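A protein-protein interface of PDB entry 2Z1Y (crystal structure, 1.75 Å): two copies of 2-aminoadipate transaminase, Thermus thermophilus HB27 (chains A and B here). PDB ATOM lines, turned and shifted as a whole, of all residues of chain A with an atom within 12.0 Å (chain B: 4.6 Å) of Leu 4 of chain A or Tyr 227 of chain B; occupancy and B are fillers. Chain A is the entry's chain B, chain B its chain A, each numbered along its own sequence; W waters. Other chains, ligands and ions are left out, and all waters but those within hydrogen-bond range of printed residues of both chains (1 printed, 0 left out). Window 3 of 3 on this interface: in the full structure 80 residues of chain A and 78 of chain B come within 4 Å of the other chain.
O of Leu 197 of chain B sits at hydrogen-bond distance from OH of Tyr 227 of chain B, at 2.6 Å. N of Tyr 227 of chain B sits at hydrogen-bond distance from O of Ala 222 of chain B (2.8 Å).
Hydrophobic or aromatic side chains of chain B that line the printed part of chain A: Val 198 and Tyr 227. Of the 9 printed residues of chain A, 2 touch a printed residue of chain B. Among the printed residues, 5 pairs touch across the chains. Among the printed residues, no Asp or Glu carboxylate lies within 4 Å of a Lys or Arg side-chain nitrogen of the other chain.
Water W1 lies within hydrogen-bond range of the backbone carbonyl oxygen of Gly 196 of chain B (2.7 Å) and the backbone NH of Ser 5 of chain A (3.0 Å).
Leu 4 of chain A touches Gly 196 of chain B. CD1 of Leu 4 of chain A touches OH of Tyr 227 of chain B, at 3.6 Å. Leu 4 of chain A touches Gly 229 of chain B (CD1 to CA, 3.4 Å). CG2 of Val 198 of chain B touches CZ3 of Trp 6 of chain A, at 3.8 Å. Trp 6 of chain A touches Pro 228 of chain B.
No position is printed for both chains.
Of chain B, only Gly 196, Tyr 227 and Gly 229 come within 4 Å of Leu 4 of chain A. Of the printed residues of chain B, Trp 6 of chain A touches Val 198 (3.8 Å) and Pro 228 (3.2 Å). Leu 189 of chain B touches none of the printed residues of chain A. Gly 196 of chain B touches just one residue of chain A: Leu 4 (3.9 Å). Ala 222 of chain B touches none of the printed residues of chain A. No residue of chain A comes within 4 Å of Ala 225 of chain B. Tyr 227 of chain B touches one residue of chain A. Gly 229 of chain B touches just one residue of chain A: Leu 4 (3.4 Å). The nearest residue of chain A that does not touch Tyr 227 of chain B is Pro 3 of chain A (6.4 Å). The nearest printed residue of chain B that does not touch Trp 6 of chain A is Gly 229 of chain B (4.1 Å).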
ATOM      1  N   PRO A   3     -16.516  -0.125 -24.639  1.00  0.00           N
ATOM      2  CA  PRO A   3     -17.350   1.082 -24.542  1.00  0.00           C
ATOM      3  C   PRO A   3     -18.762   0.581 -24.799  1.00  0.00           C
ATOM      4  O   PRO A   3     -18.965  -0.211 -25.712  1.00  0.00           O
ATOM      5  CB  PRO A   3     -16.922   2.090 -25.621  1.00  0.00           C
ATOM      6  CG  PRO A   3     -15.999   1.286 -26.482  1.00  0.00           C
ATOM      7  CD  PRO A   3     -15.999  -0.168 -25.981  1.00  0.00           C
ATOM      8  N   LEU A   4     -19.716   0.972 -23.944  1.00  0.00           N
ATOM      9  CA  LEU A   4     -21.022   0.343 -23.952  1.00  0.00           C
ATOM     10  C   LEU A   4     -21.721   0.650 -25.273  1.00  0.00           C
ATOM     11  O   LEU A   4     -21.652   1.804 -25.717  1.00  0.00           O
ATOM     12  CB  LEU A   4     -21.794   0.904 -22.755  1.00  0.00           C
ATOM     13  CG  LEU A   4     -23.264   0.462 -22.646  1.00  0.00           C
ATOM     14  CD1 LEU A   4     -23.719   0.389 -21.203  1.00  0.00           C
ATOM     15  CD2 LEU A   4     -24.170   1.363 -23.378  1.00  0.00           C
ATOM     16  N   SER A   5     -22.494  -0.311 -25.846  1.00  0.00           N
ATOM     17  CA  SER A   5     -23.258  -0.016 -27.042  1.00  0.00           C
ATOM     18  C   SER A   5     -24.770  -0.046 -26.808  1.00  0.00           C
ATOM     19  O   SER A   5     -25.324  -1.120 -26.624  1.00  0.00           O
ATOM     20  CB  SER A   5     -22.975  -1.008 -28.175  1.00  0.00           C
ATOM     21  OG  SER A   5     -23.957  -0.836 -29.202  1.00  0.00           O
ATOM     22  N   TRP A   6     -25.443   1.117 -26.851  1.00  0.00           N
ATOM     23  CA  TRP A   6     -26.890   1.121 -26.630  1.00  0.00           C
ATOM     24  C   TRP A   6     -27.608   0.372 -27.739  1.00  0.00           C
ATOM     25  O   TRP A   6     -28.492  -0.475 -27.468  1.00  0.00           O
ATOM     26  CB  TRP A   6     -27.446   2.540 -26.456  1.00  0.00           C
ATOM     27  CG  TRP A   6     -27.093   3.090 -25.110  1.00  0.00           C
ATOM     28  CD1 TRP A   6     -26.173   4.035 -24.846  1.00  0.00           C
ATOM     29  CD2 TRP A   6     -27.575   2.615 -23.833  1.00  0.00           C
ATOM     30  NE1 TRP A   6     -26.115   4.262 -23.518  1.00  0.00           N
ATOM     31  CE2 TRP A   6     -26.919   3.387 -22.856  1.00  0.00           C
ATOM     32  CE3 TRP A   6     -28.482   1.618 -23.433  1.00  0.00           C
ATOM     33  CZ2 TRP A   6     -27.153   3.239 -21.492  1.00  0.00           C
ATOM     34  CZ3 TRP A   6     -28.632   1.401 -22.078  1.00  0.00           C
ATOM     35  CH2 TRP A   6     -27.992   2.215 -21.126  1.00  0.00           C
ATOM     36  N   SER A   7     -27.215   0.628 -28.983  1.00  0.00           N
ATOM     37  CA  SER A   7     -28.005   0.076 -30.101  1.00  0.00           C
ATOM     38  C   SER A   7     -27.998  -1.446 -30.068  1.00  0.00           C
ATOM     39  O   SER A   7     -29.026  -2.077 -30.325  1.00  0.00           O
ATOM     40  CB  SER A   7     -27.531   0.520 -31.456  1.00  0.00           C
ATOM     41  OG  SER A   7     -26.140   0.312 -31.561  1.00  0.00           O
ATOM     42  N   GLU A   8     -26.843  -2.030 -29.725  1.00  0.00           N
ATOM     43  CA  GLU A   8     -26.734  -3.472 -29.552  1.00  0.00           C
ATOM     44  C   GLU A   8     -27.458  -3.991 -28.297  1.00  0.00           C
ATOM     45  O   GLU A   8     -27.796  -5.151 -28.280  1.00  0.00           O
ATOM     46  CB  GLU A   8     -25.280  -3.956 -29.509  1.00  0.00           C
ATOM     47  CG  GLU A   8     -24.528  -3.789 -30.828  1.00  0.00           C
ATOM     48  CD  GLU A   8     -23.006  -3.925 -30.692  1.00  0.00           C
ATOM     49  OE1 GLU A   8     -22.503  -4.423 -29.671  1.00  0.00           O
ATOM     50  OE2 GLU A   8     -22.300  -3.450 -31.599  1.00  0.00           O
ATOM     51  N   ALA A   9     -27.714  -3.167 -27.264  1.00  0.00           N
ATOM     52  CA  ALA A   9     -28.352  -3.614 -26.027  1.00  0.00           C
ATOM     53  C   ALA A   9     -29.887  -3.730 -26.095  1.00  0.00           C
ATOM     54  O   ALA A   9     -30.498  -4.513 -25.383  1.00  0.00           O
ATOM     55  CB  ALA A   9     -27.993  -2.629 -24.926  1.00  0.00           C
ATOM     56  N   PHE A  10     -30.516  -2.891 -26.914  1.00  0.00           N
ATOM     57  CA  PHE A  10     -31.965  -2.876 -27.084  1.00  0.00           C
ATOM     58  C   PHE A  10     -32.468  -4.160 -27.704  1.00  0.00           C
ATOM     59  O   PHE A  10     -31.755  -4.847 -28.471  1.00  0.00           O
ATOM     60  CB  PHE A  10     -32.351  -1.686 -27.959  1.00  0.00           C
ATOM     61  CG  PHE A  10     -31.964  -0.307 -27.474  1.00  0.00           C
ATOM     62  CD1 PHE A  10     -32.023   0.015 -26.129  1.00  0.00           C
ATOM     63  CD2 PHE A  10     -31.530   0.657 -28.366  1.00  0.00           C
ATOM     64  CE1 PHE A  10     -31.784   1.291 -25.693  1.00  0.00           C
ATOM     65  CE2 PHE A  10     -31.201   1.925 -27.920  1.00  0.00           C
ATOM     66  CZ  PHE A  10     -31.302   2.230 -26.567  1.00  0.00           C
ATOM     67  N   GLY A  11     -33.755  -4.446 -27.446  1.00  0.00           N
ATOM     68  CA  GLY A  11     -34.451  -5.532 -28.077  1.00  0.00           C
ATOM     69  C   GLY A  11     -35.272  -5.068 -29.282  1.00  0.00           C
ATOM     70  O   GLY A  11     -35.171  -3.940 -29.669  1.00  0.00           O
ATOM     71  N   LEU B 189     -20.191  -2.908  -9.764  1.00  0.00           N
ATOM     72  CA  LEU B 189     -20.006  -1.960 -10.850  1.00  0.00           C
ATOM     73  C   LEU B 189     -18.856  -2.366 -11.757  1.00  0.00           C
ATOM     74  O   LEU B 189     -18.935  -2.239 -13.002  1.00  0.00           O
ATOM     75  CB  LEU B 189     -19.782  -0.558 -10.295  1.00  0.00           C
ATOM     76  CG  LEU B 189     -19.521   0.537 -11.329  1.00  0.00           C
ATOM     77  CD1 LEU B 189     -20.746   0.741 -12.226  1.00  0.00           C
ATOM     78  CD2 LEU B 189     -19.013   1.786 -10.674  1.00  0.00           C
ATOM     79  N   VAL B 192     -19.939  -5.239 -14.063  1.00  0.00           N
ATOM     80  CA  VAL B 192     -20.757  -4.720 -15.142  1.00  0.00           C
ATOM     81  C   VAL B 192     -19.919  -3.906 -16.124  1.00  0.00           C
ATOM     82  O   VAL B 192     -20.080  -4.037 -17.338  1.00  0.00           O
ATOM     83  CB  VAL B 192     -21.844  -3.897 -14.415  1.00  0.00           C
ATOM     84  CG1 VAL B 192     -22.314  -2.748 -15.231  1.00  0.00           C
ATOM     85  CG2 VAL B 192     -22.970  -4.807 -13.854  1.00  0.00           C
ATOM     86  N   MET B 193     -18.996  -3.086 -15.655  1.00  0.00           N
ATOM     87  CA  MET B 193     -18.281  -2.266 -16.601  1.00  0.00           C
ATOM     88  C   MET B 193     -17.344  -3.120 -17.461  1.00  0.00           C
ATOM     89  O   MET B 193     -17.070  -2.770 -18.607  1.00  0.00           O
ATOM     90  CB  MET B 193     -17.459  -1.185 -15.900  1.00  0.00           C
ATOM     91  CG  MET B 193     -18.311  -0.174 -15.191  1.00  0.00           C
ATOM     92  SD  MET B 193     -17.393   1.183 -14.425  1.00  0.00           S
ATOM     93  CE  MET B 193     -16.165   0.404 -13.381  1.00  0.00           C
ATOM     94  N   GLY B 196     -19.476  -4.213 -20.265  1.00  0.00           N
ATOM     95  CA  GLY B 196     -20.398  -3.215 -20.810  1.00  0.00           C
ATOM     96  C   GLY B 196     -21.891  -3.568 -20.645  1.00  0.00           C
ATOM     97  O   GLY B 196     -22.695  -3.376 -21.570  1.00  0.00           O
ATOM     98  N   LEU B 197     -22.259  -4.049 -19.466  1.00  0.00           N
ATOM     99  CA  LEU B 197     -23.618  -4.479 -19.193  1.00  0.00           C
ATOM    100  C   LEU B 197     -24.464  -3.295 -18.726  1.00  0.00           C
ATOM    101  O   LEU B 197     -23.993  -2.301 -18.171  1.00  0.00           O
ATOM    102  CB  LEU B 197     -23.544  -5.561 -18.129  1.00  0.00           C
ATOM    103  CG  LEU B 197     -22.899  -6.881 -18.557  1.00  0.00           C
ATOM    104  CD1 LEU B 197     -22.694  -7.790 -17.388  1.00  0.00           C
ATOM    105  CD2 LEU B 197     -23.736  -7.560 -19.572  1.00  0.00           C
ATOM    106  N   VAL B 198     -25.760  -3.459 -18.879  1.00  0.00           N
ATOM    107  CA  VAL B 198     -26.763  -2.483 -18.476  1.00  0.00           C
ATOM    108  C   VAL B 198     -27.310  -2.938 -17.126  1.00  0.00           C
ATOM    109  O   VAL B 198     -27.641  -4.067 -16.933  1.00  0.00           O
ATOM    110  CB  VAL B 198     -27.913  -2.374 -19.508  1.00  0.00           C
ATOM    111  CG1 VAL B 198     -28.942  -1.367 -18.998  1.00  0.00           C
ATOM    112  CG2 VAL B 198     -27.410  -2.020 -20.917  1.00  0.00           C
ATOM    113  N   ALA B 222     -21.407   4.804 -10.934  1.00  0.00           N
ATOM    114  CA  ALA B 222     -21.197   4.735 -12.379  1.00  0.00           C
ATOM    115  C   ALA B 222     -20.857   6.113 -12.948  1.00  0.00           C
ATOM    116  O   ALA B 222     -19.899   6.242 -13.699  1.00  0.00           O
ATOM    117  CB  ALA B 222     -22.434   4.162 -13.067  1.00  0.00           C
ATOM    118  N   ARG B 223     -21.607   7.150 -12.545  1.00  0.00           N
ATOM    119  CA  ARG B 223     -21.382   8.528 -12.981  1.00  0.00           C
ATOM    120  C   ARG B 223     -19.957   8.945 -12.611  1.00  0.00           C
ATOM    121  O   ARG B 223     -19.214   9.473 -13.433  1.00  0.00           O
ATOM    122  CB  ARG B 223     -22.470   9.440 -12.399  1.00  0.00           C
ATOM    123  CG  ARG B 223     -22.548  10.847 -12.976  1.00  0.00           C
ATOM    124  CD  ARG B 223     -22.814  11.977 -11.952  1.00  0.00           C
ATOM    125  NE  ARG B 223     -24.180  12.158 -11.453  1.00  0.00           N
ATOM    126  CZ  ARG B 223     -24.599  12.053 -10.151  1.00  0.00           C
ATOM    127  NH1 ARG B 223     -25.867  12.228  -9.866  1.00  0.00           N
ATOM    128  NH2 ARG B 223     -23.802  11.813  -9.120  1.00  0.00           N
ATOM    129  N   ALA B 225     -17.341   7.023 -12.299  1.00  0.00           N
ATOM    130  CA  ALA B 225     -16.486   6.215 -13.128  1.00  0.00           C
ATOM    131  C   ALA B 225     -16.593   6.602 -14.609  1.00  0.00           C
ATOM    132  O   ALA B 225     -15.898   6.023 -15.416  1.00  0.00           O
ATOM    133  CB  ALA B 225     -16.866   4.759 -12.980  1.00  0.00           C
ATOM    134  N   GLY B 226     -17.518   7.454 -14.968  1.00  0.00           N
ATOM    135  CA  GLY B 226     -17.762   7.831 -16.350  1.00  0.00           C
ATOM    136  C   GLY B 226     -18.523   6.746 -17.135  1.00  0.00           C
ATOM    137  O   GLY B 226     -18.548   6.730 -18.357  1.00  0.00           O
ATOM    138  N   TYR B 227     -19.199   5.856 -16.430  1.00  0.00           N
ATOM    139  CA  TYR B 227     -19.835   4.701 -17.046  1.00  0.00           C
ATOM    140  C   TYR B 227     -21.323   5.002 -17.281  1.00  0.00           C
ATOM    141  O   TYR B 227     -22.010   5.465 -16.348  1.00  0.00           O
ATOM    142  CB  TYR B 227     -19.685   3.453 -16.160  1.00  0.00           C
ATOM    143  CG  TYR B 227     -20.299   2.217 -16.809  1.00  0.00           C
ATOM    144  CD1 TYR B 227     -19.675   1.647 -17.907  1.00  0.00           C
ATOM    145  CD2 TYR B 227     -21.436   1.562 -16.313  1.00  0.00           C
ATOM    146  CE1 TYR B 227     -20.185   0.549 -18.576  1.00  0.00           C
ATOM    147  CE2 TYR B 227     -21.959   0.450 -16.984  1.00  0.00           C
ATOM    148  CZ  TYR B 227     -21.326  -0.056 -18.116  1.00  0.00           C
ATOM    149  OH  TYR B 227     -21.667  -1.211 -18.742  1.00  0.00           O
ATOM    150  N   PRO B 228     -21.829   4.868 -18.551  1.00  0.00           N
ATOM    151  CA  PRO B 228     -23.206   5.276 -18.891  1.00  0.00           C
ATOM    152  C   PRO B 228     -24.304   4.210 -18.769  1.00  0.00           C
ATOM    153  O   PRO B 228     -25.426   4.493 -19.106  1.00  0.00           O
ATOM    154  CB  PRO B 228     -23.046   5.642 -20.347  1.00  0.00           C
ATOM    155  CG  PRO B 228     -22.135   4.640 -20.887  1.00  0.00           C
ATOM    156  CD  PRO B 228     -21.059   4.478 -19.759  1.00  0.00           C
ATOM    157  N   GLY B 229     -23.986   3.030 -18.248  1.00  0.00           N
ATOM    158  CA  GLY B 229     -24.856   1.856 -18.334  1.00  0.00           C
ATOM    159  C   GLY B 229     -25.864   1.675 -17.206  1.00  0.00           C
ATOM    160  O   GLY B 229     -26.524   0.644 -17.172  1.00  0.00           O
HETATM  161  O   HOH W   1     -22.280  -2.829 -24.182  1.00  0.00           O
